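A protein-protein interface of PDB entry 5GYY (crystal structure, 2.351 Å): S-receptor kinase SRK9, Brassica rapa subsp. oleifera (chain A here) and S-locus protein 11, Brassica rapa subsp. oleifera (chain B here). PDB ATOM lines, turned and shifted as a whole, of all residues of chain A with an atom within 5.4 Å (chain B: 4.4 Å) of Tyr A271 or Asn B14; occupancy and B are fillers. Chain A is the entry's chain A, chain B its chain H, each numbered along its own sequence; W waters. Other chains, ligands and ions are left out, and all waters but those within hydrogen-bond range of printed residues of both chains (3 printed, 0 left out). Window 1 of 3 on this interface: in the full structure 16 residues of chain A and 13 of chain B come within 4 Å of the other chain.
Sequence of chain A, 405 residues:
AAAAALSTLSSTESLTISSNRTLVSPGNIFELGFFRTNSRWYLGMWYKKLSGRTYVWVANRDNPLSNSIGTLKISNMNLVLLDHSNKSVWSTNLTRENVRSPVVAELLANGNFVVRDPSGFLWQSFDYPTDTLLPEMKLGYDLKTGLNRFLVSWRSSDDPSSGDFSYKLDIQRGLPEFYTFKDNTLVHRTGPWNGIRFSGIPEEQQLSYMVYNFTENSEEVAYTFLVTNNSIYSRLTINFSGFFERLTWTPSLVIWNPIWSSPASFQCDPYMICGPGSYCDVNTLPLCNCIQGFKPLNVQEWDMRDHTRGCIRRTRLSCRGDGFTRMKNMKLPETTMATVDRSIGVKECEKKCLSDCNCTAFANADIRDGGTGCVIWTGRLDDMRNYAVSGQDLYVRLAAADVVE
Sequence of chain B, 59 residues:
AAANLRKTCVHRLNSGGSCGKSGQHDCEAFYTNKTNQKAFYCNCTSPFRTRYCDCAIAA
Among the printed residues, pairs that only touch across the chains: Leu A186 with Tyr B52, Pro A270 with Tyr B52, Tyr A271 with Arg B12 and Thr A308 with Leu B13.
The side-chain hydroxyl (OH) of Tyr A271 is in hydrogen-bond range of the side-chain carboxylate (OE1) of Glu A334 (2.7 Å). O of Leu B13 sits at hydrogen-bond distance from N of Cys B53, at 2.9 Å. The backbone carbonyl oxygen (O) of Val A187 sits at hydrogen-bond distance from the backbone NH (N) of Tyr A271, 3.0 Å away.
Water W3 lies within hydrogen-bond range of NE of Arg B12 (2.6 Å) and N of Leu A186 (2.8 Å). Water W2 bridges O of Asn B14 (2.6 Å) and OG1 of Thr A308 (2.9 Å). Water W1 lies within hydrogen-bond range of the backbone carbonyl oxygen (O) of Leu A186 and the side-chain amide nitrogen (ND2) of Asn B14.
The backbone carbonyl oxygen (O) of Tyr A271 sits at hydrogen-bond distance from the side-chain amide nitrogen (ND2) of Asn B14 (2.8 Å). O of Val A187 is in hydrogen-bond range of OH of Tyr B52 (2.7 Å).
Of the printed residues of chain B, Leu A186 touches Tyr B52. Tyr A271 touches just these residues of chain B: Arg B12 (3.8 Å) and Asn B14 (2.8 Å). Printed residues of chain B within 4 Å of Thr A308: Leu B13. Of the printed residues of chain A, Arg B12 touches Tyr A271 (3.8 Å). Of the printed residues of chain A, Leu B13 touches Thr A308. Asn B14 touches one residue of chain A. The nearest residue of chain B that does not touch Tyr A271 is Tyr B52 (4.1 Å).
Of the 13 printed residues of chain A, 5 touch a printed residue of chain B. Printed residues of chain A that touch a printed residue of chain B: Leu A186, Val A187, Pro A270, Tyr A271 and Thr A308. Hydrophobic or aromatic side chains of chain A within 4 Å of the printed part of chain B: Val A187, Pro A270 and Tyr A271. Of the 7 printed residues of chain B, 4 touch a printed residue of chain A. Printed residues of chain B that touch a printed residue of chain A: Arg B12, Leu B13, Asn B14 and Tyr B52. Among the printed residues, no Asp or Glu carboxylate lies within 4 Å of a Lys or Arg side-chain nitrogen of the other chain.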
ATOM      1  N   TYR A 179     -18.568  -3.825  30.786  1.00  0.00           N
ATOM      2  CA  TYR A 179     -17.213  -3.432  30.439  1.00  0.00           C
ATOM      3  C   TYR A 179     -16.203  -4.078  31.384  1.00  0.00           C
ATOM      4  O   TYR A 179     -16.529  -4.360  32.545  1.00  0.00           O
ATOM      5  CB  TYR A 179     -17.058  -1.913  30.563  1.00  0.00           C
ATOM      6  CG  TYR A 179     -17.692  -1.130  29.449  1.00  0.00           C
ATOM      7  CD1 TYR A 179     -16.973  -0.810  28.310  1.00  0.00           C
ATOM      8  CD2 TYR A 179     -19.017  -0.711  29.531  1.00  0.00           C
ATOM      9  CE1 TYR A 179     -17.553  -0.091  27.273  1.00  0.00           C
ATOM     10  CE2 TYR A 179     -19.610   0.012  28.500  1.00  0.00           C
ATOM     11  CZ  TYR A 179     -18.873   0.324  27.382  1.00  0.00           C
ATOM     12  OH  TYR A 179     -19.458   1.039  26.363  1.00  0.00           O
ATOM     13  N   LEU A 186     -10.370   1.555  29.993  1.00  0.00           N
ATOM     14  CA  LEU A 186     -11.397   0.699  29.421  1.00  0.00           C
ATOM     15  C   LEU A 186     -10.672  -0.341  28.562  1.00  0.00           C
ATOM     16  O   LEU A 186     -10.071   0.012  27.551  1.00  0.00           O
ATOM     17  CB  LEU A 186     -12.349   1.546  28.573  1.00  0.00           C
ATOM     18  CG  LEU A 186     -13.772   1.037  28.394  1.00  0.00           C
ATOM     19  CD1 LEU A 186     -14.659   2.137  27.800  1.00  0.00           C
ATOM     20  CD2 LEU A 186     -13.778  -0.209  27.511  1.00  0.00           C
ATOM     21  N   VAL A 187     -10.690  -1.607  28.968  1.00  0.00           N
ATOM     22  CA  VAL A 187      -9.845  -2.592  28.255  1.00  0.00           C
ATOM     23  C   VAL A 187     -10.592  -3.578  27.390  1.00  0.00           C
ATOM     24  O   VAL A 187     -10.067  -4.035  26.381  1.00  0.00           O
ATOM     25  CB  VAL A 187      -8.853  -3.352  29.185  1.00  0.00           C
ATOM     26  CG1 VAL A 187      -7.811  -2.386  29.749  1.00  0.00           C
ATOM     27  CG2 VAL A 187      -9.581  -4.079  30.307  1.00  0.00           C
ATOM     28  N   HIS A 188     -11.819  -3.902  27.779  1.00  0.00           N
ATOM     29  CA  HIS A 188     -12.677  -4.767  26.969  1.00  0.00           C
ATOM     30  C   HIS A 188     -14.137  -4.416  27.167  1.00  0.00           C
ATOM     31  O   HIS A 188     -14.556  -4.045  28.255  1.00  0.00           O
ATOM     32  CB  HIS A 188     -12.462  -6.252  27.297  1.00  0.00           C
ATOM     33  CG  HIS A 188     -13.390  -7.174  26.568  1.00  0.00           C
ATOM     34  ND1 HIS A 188     -14.462  -7.791  27.180  1.00  0.00           N
ATOM     35  CD2 HIS A 188     -13.418  -7.574  25.271  1.00  0.00           C
ATOM     36  CE1 HIS A 188     -15.111  -8.529  26.291  1.00  0.00           C
ATOM     37  NE2 HIS A 188     -14.495  -8.418  25.128  1.00  0.00           N
ATOM     38  N   ARG A 189     -14.908  -4.584  26.109  1.00  0.00           N
ATOM     39  CA  ARG A 189     -16.322  -4.279  26.131  1.00  0.00           C
ATOM     40  C   ARG A 189     -17.151  -5.525  25.838  1.00  0.00           C
ATOM     41  O   ARG A 189     -17.225  -5.976  24.700  1.00  0.00           O
ATOM     42  CB  ARG A 189     -16.593  -3.210  25.072  1.00  0.00           C
ATOM     43  CG  ARG A 189     -18.050  -2.780  24.929  1.00  0.00           C
ATOM     44  CD  ARG A 189     -18.234  -1.986  23.641  1.00  0.00           C
ATOM     45  NE  ARG A 189     -19.526  -2.312  23.091  1.00  0.00           N
ATOM     46  CZ  ARG A 189     -19.744  -2.734  21.854  1.00  0.00           C
ATOM     47  NH1 ARG A 189     -18.751  -2.855  20.980  1.00  0.00           N
ATOM     48  NH2 ARG A 189     -20.986  -3.011  21.489  1.00  0.00           N
ATOM     49  N   ASP A 269     -10.766  -9.081  20.355  1.00  0.00           N
ATOM     50  CA  ASP A 269     -11.608  -8.659  21.479  1.00  0.00           C
ATOM     51  C   ASP A 269     -11.183  -7.386  22.226  1.00  0.00           C
ATOM     52  O   ASP A 269     -12.052  -6.674  22.742  1.00  0.00           O
ATOM     53  CB  ASP A 269     -11.816  -9.798  22.476  1.00  0.00           C
ATOM     54  CG  ASP A 269     -12.807 -10.840  21.983  1.00  0.00           C
ATOM     55  OD1 ASP A 269     -13.742 -10.480  21.233  1.00  0.00           O
ATOM     56  OD2 ASP A 269     -12.641 -12.024  22.348  1.00  0.00           O
ATOM     57  N   PRO A 270      -9.864  -7.089  22.304  1.00  0.00           N
ATOM     58  CA  PRO A 270      -9.546  -5.843  23.023  1.00  0.00           C
ATOM     59  C   PRO A 270     -10.263  -4.581  22.507  1.00  0.00           C
ATOM     60  O   PRO A 270     -10.507  -4.411  21.315  1.00  0.00           O
ATOM     61  CB  PRO A 270      -8.026  -5.727  22.856  1.00  0.00           C
ATOM     62  CG  PRO A 270      -7.570  -7.127  22.799  1.00  0.00           C
ATOM     63  CD  PRO A 270      -8.647  -7.882  22.046  1.00  0.00           C
ATOM     64  N   TYR A 271     -10.607  -3.704  23.438  1.00  0.00           N
ATOM     65  CA  TYR A 271     -11.396  -2.520  23.127  1.00  0.00           C
ATOM     66  C   TYR A 271     -10.745  -1.646  22.053  1.00  0.00           C
ATOM     67  O   TYR A 271      -9.615  -1.158  22.216  1.00  0.00           O
ATOM     68  CB  TYR A 271     -11.659  -1.715  24.402  1.00  0.00           C
ATOM     69  CG  TYR A 271     -12.571  -0.540  24.221  1.00  0.00           C
ATOM     70  CD1 TYR A 271     -13.882  -0.713  23.792  1.00  0.00           C
ATOM     71  CD2 TYR A 271     -12.131   0.746  24.498  1.00  0.00           C
ATOM     72  CE1 TYR A 271     -14.723   0.366  23.630  1.00  0.00           C
ATOM     73  CE2 TYR A 271     -12.961   1.830  24.345  1.00  0.00           C
ATOM     74  CZ  TYR A 271     -14.259   1.638  23.911  1.00  0.00           C
ATOM     75  OH  TYR A 271     -15.090   2.717  23.756  1.00  0.00           O
ATOM     76  N   MET A 272     -11.464  -1.486  20.944  1.00  0.00           N
ATOM     77  CA  MET A 272     -10.996  -0.705  19.797  1.00  0.00           C
ATOM     78  C   MET A 272      -9.598  -1.064  19.249  1.00  0.00           C
ATOM     79  O   MET A 272      -8.799  -0.174  18.976  1.00  0.00           O
ATOM     80  CB  MET A 272     -11.090   0.790  20.108  1.00  0.00           C
ATOM     81  CG  MET A 272     -12.470   1.196  20.657  1.00  0.00           C
ATOM     82  SD  MET A 272     -12.885   2.939  20.450  1.00  0.00           S
ATOM     83  CE  MET A 272     -11.362   3.744  20.970  1.00  0.00           C
ATOM     84  N   ILE A 273      -9.290  -2.346  19.077  1.00  0.00           N
ATOM     85  CA  ILE A 273      -8.041  -2.677  18.373  1.00  0.00           C
ATOM     86  C   ILE A 273      -8.101  -2.173  16.935  1.00  0.00           C
ATOM     87  O   ILE A 273      -7.065  -1.899  16.335  1.00  0.00           O
ATOM     88  CB  ILE A 273      -7.658  -4.185  18.375  1.00  0.00           C
ATOM     89  CG1 ILE A 273      -8.830  -5.056  18.810  1.00  0.00           C
ATOM     90  CG2 ILE A 273      -6.382  -4.429  19.206  1.00  0.00           C
ATOM     91  CD1 ILE A 273      -9.925  -5.152  17.768  1.00  0.00           C
ATOM     92  N   THR A 308      -5.315   2.631  13.618  1.00  0.00           N
ATOM     93  CA  THR A 308      -5.787   3.588  14.623  1.00  0.00           C
ATOM     94  C   THR A 308      -6.844   4.555  14.093  1.00  0.00           C
ATOM     95  O   THR A 308      -7.914   4.696  14.691  1.00  0.00           O
ATOM     96  CB  THR A 308      -4.613   4.442  15.176  1.00  0.00           C
ATOM     97  OG1 THR A 308      -3.451   3.624  15.372  1.00  0.00           O
ATOM     98  CG2 THR A 308      -4.999   5.118  16.479  1.00  0.00           C
ATOM     99  N   GLU A 334     -20.445   0.027  19.964  1.00  0.00           N
ATOM    100  CA  GLU A 334     -20.739   0.577  21.270  1.00  0.00           C
ATOM    101  C   GLU A 334     -21.951   1.480  21.114  1.00  0.00           C
ATOM    102  O   GLU A 334     -22.050   2.176  20.104  1.00  0.00           O
ATOM    103  CB  GLU A 334     -19.543   1.368  21.758  1.00  0.00           C
ATOM    104  CG  GLU A 334     -19.573   1.664  23.219  1.00  0.00           C
ATOM    105  CD  GLU A 334     -18.270   2.263  23.684  1.00  0.00           C
ATOM    106  OE1 GLU A 334     -17.593   2.884  22.839  1.00  0.00           O
ATOM    107  OE2 GLU A 334     -17.937   2.124  24.879  1.00  0.00           O
ATOM    108  N   ASP A 383     -15.447  -0.085  17.915  1.00  0.00           N
ATOM    109  CA  ASP A 383     -15.197  -1.320  18.652  1.00  0.00           C
ATOM    110  C   ASP A 383     -15.923  -2.530  18.089  1.00  0.00           C
ATOM    111  O   ASP A 383     -16.454  -3.357  18.819  1.00  0.00           O
ATOM    112  CB  ASP A 383     -15.459  -1.132  20.162  1.00  0.00           C
ATOM    113  CG  ASP A 383     -15.010  -2.329  20.995  1.00  0.00           C
ATOM    114  OD1 ASP A 383     -13.867  -2.806  20.772  1.00  0.00           O
ATOM    115  OD2 ASP A 383     -15.792  -2.788  21.871  1.00  0.00           O
ATOM    116  N   ARG B  12      -8.025   8.281  23.879  1.00  0.00           N
ATOM    117  CA  ARG B  12      -7.758   6.872  24.038  1.00  0.00           C
ATOM    118  C   ARG B  12      -7.203   6.297  22.730  1.00  0.00           C
ATOM    119  O   ARG B  12      -7.823   6.427  21.676  1.00  0.00           O
ATOM    120  CB  ARG B  12      -9.087   6.253  24.466  1.00  0.00           C
ATOM    121  CG  ARG B  12      -9.108   4.840  24.895  1.00  0.00           C
ATOM    122  CD  ARG B  12     -10.516   4.494  25.428  1.00  0.00           C
ATOM    123  NE  ARG B  12     -10.877   5.169  26.676  1.00  0.00           N
ATOM    124  CZ  ARG B  12     -12.079   5.688  26.914  1.00  0.00           C
ATOM    125  NH1 ARG B  12     -13.024   5.610  25.984  1.00  0.00           N
ATOM    126  NH2 ARG B  12     -12.343   6.286  28.071  1.00  0.00           N
ATOM    127  N   LEU B  13      -6.012   5.696  22.801  1.00  0.00           N
ATOM    128  CA  LEU B  13      -5.345   5.095  21.634  1.00  0.00           C
ATOM    129  C   LEU B  13      -4.752   3.715  21.937  1.00  0.00           C
ATOM    130  O   LEU B  13      -3.810   3.600  22.728  1.00  0.00           O
ATOM    131  CB  LEU B  13      -4.243   6.007  21.100  1.00  0.00           C
ATOM    132  CG  LEU B  13      -4.677   7.378  20.595  1.00  0.00           C
ATOM    133  CD1 LEU B  13      -3.468   8.236  20.264  1.00  0.00           C
ATOM    134  CD2 LEU B  13      -5.593   7.234  19.385  1.00  0.00           C
ATOM    135  N   ASN B  14      -5.299   2.683  21.297  1.00  0.00           N
ATOM    136  CA  ASN B  14      -4.922   1.299  21.573  1.00  0.00           C
ATOM    137  C   ASN B  14      -4.369   0.571  20.366  1.00  0.00           C
ATOM    138  O   ASN B  14      -4.782   0.845  19.234  1.00  0.00           O
ATOM    139  CB  ASN B  14      -6.139   0.523  22.063  1.00  0.00           C
ATOM    140  CG  ASN B  14      -6.861   1.221  23.189  1.00  0.00           C
ATOM    141  OD1 ASN B  14      -6.280   2.038  23.898  1.00  0.00           O
ATOM    142  ND2 ASN B  14      -8.123   0.869  23.390  1.00  0.00           N
ATOM    143  N   SER B  15      -3.454  -0.371  20.606  1.00  0.00           N
ATOM    144  CA  SER B  15      -2.951  -1.246  19.545  1.00  0.00           C
ATOM    145  C   SER B  15      -2.243  -2.487  20.087  1.00  0.00           C
ATOM    146  O   SER B  15      -1.935  -2.582  21.277  1.00  0.00           O
ATOM    147  CB  SER B  15      -1.993  -0.494  18.617  1.00  0.00           C
ATOM    148  OG  SER B  15      -0.838  -0.066  19.318  1.00  0.00           O
ATOM    149  N   ARG B  51      -1.435  -2.700  23.830  1.00  0.00           N
ATOM    150  CA  ARG B  51      -1.016  -1.469  24.504  1.00  0.00           C
ATOM    151  C   ARG B  51      -2.172  -0.451  24.582  1.00  0.00           C
ATOM    152  O   ARG B  51      -2.697  -0.014  23.556  1.00  0.00           O
ATOM    153  CB  ARG B  51       0.176  -0.817  23.787  1.00  0.00           C
ATOM    154  CG  ARG B  51       0.796   0.341  24.588  1.00  0.00           C
ATOM    155  CD  ARG B  51       1.838   1.145  23.811  1.00  0.00           C
ATOM    156  NE  ARG B  51       1.356   1.727  22.552  1.00  0.00           N
ATOM    157  CZ  ARG B  51       2.151   2.347  21.684  1.00  0.00           C
ATOM    158  NH1 ARG B  51       3.446   2.458  21.942  1.00  0.00           N
ATOM    159  NH2 ARG B  51       1.670   2.846  20.559  1.00  0.00           N
ATOM    160  N   TYR B  52      -2.570  -0.088  25.798  1.00  0.00           N
ATOM    161  CA  TYR B  52      -3.620   0.911  25.972  1.00  0.00           C
ATOM    162  C   TYR B  52      -3.041   2.255  26.415  1.00  0.00           C
ATOM    163  O   TYR B  52      -2.608   2.409  27.560  1.00  0.00           O
ATOM    164  CB  TYR B  52      -4.657   0.457  27.002  1.00  0.00           C
ATOM    165  CG  TYR B  52      -5.389  -0.828  26.672  1.00  0.00           C
ATOM    166  CD1 TYR B  52      -6.633  -0.804  26.059  1.00  0.00           C
ATOM    167  CD2 TYR B  52      -4.840  -2.062  26.996  1.00  0.00           C
ATOM    168  CE1 TYR B  52      -7.310  -1.969  25.774  1.00  0.00           C
ATOM    169  CE2 TYR B  52      -5.502  -3.229  26.724  1.00  0.00           C
ATOM    170  CZ  TYR B  52      -6.741  -3.189  26.110  1.00  0.00           C
ATOM    171  OH  TYR B  52      -7.399  -4.376  25.823  1.00  0.00           O
ATOM    172  N   CYS B  53      -3.062   3.233  25.518  1.00  0.00           N
ATOM    173  CA  CYS B  53      -2.656   4.583  25.881  1.00  0.00           C
ATOM    174  C   CYS B  53      -3.882   5.398  26.317  1.00  0.00           C
ATOM    175  O   CYS B  53      -4.864   5.521  25.571  1.00  0.00           O
ATOM    176  CB  CYS B  53      -1.951   5.279  24.709  1.00  0.00           C
ATOM    177  SG  CYS B  53      -0.465   4.448  24.094  1.00  0.00           S
HETATM  178  O   HOH W   1      -9.163   1.998  26.082  1.00  0.00           O
HETATM  179  O   HOH W   2      -4.406   1.226  16.663  1.00  0.00           O
HETATM  180  O   HOH W   3      -9.826   3.972  28.751  1.00  0.00           O
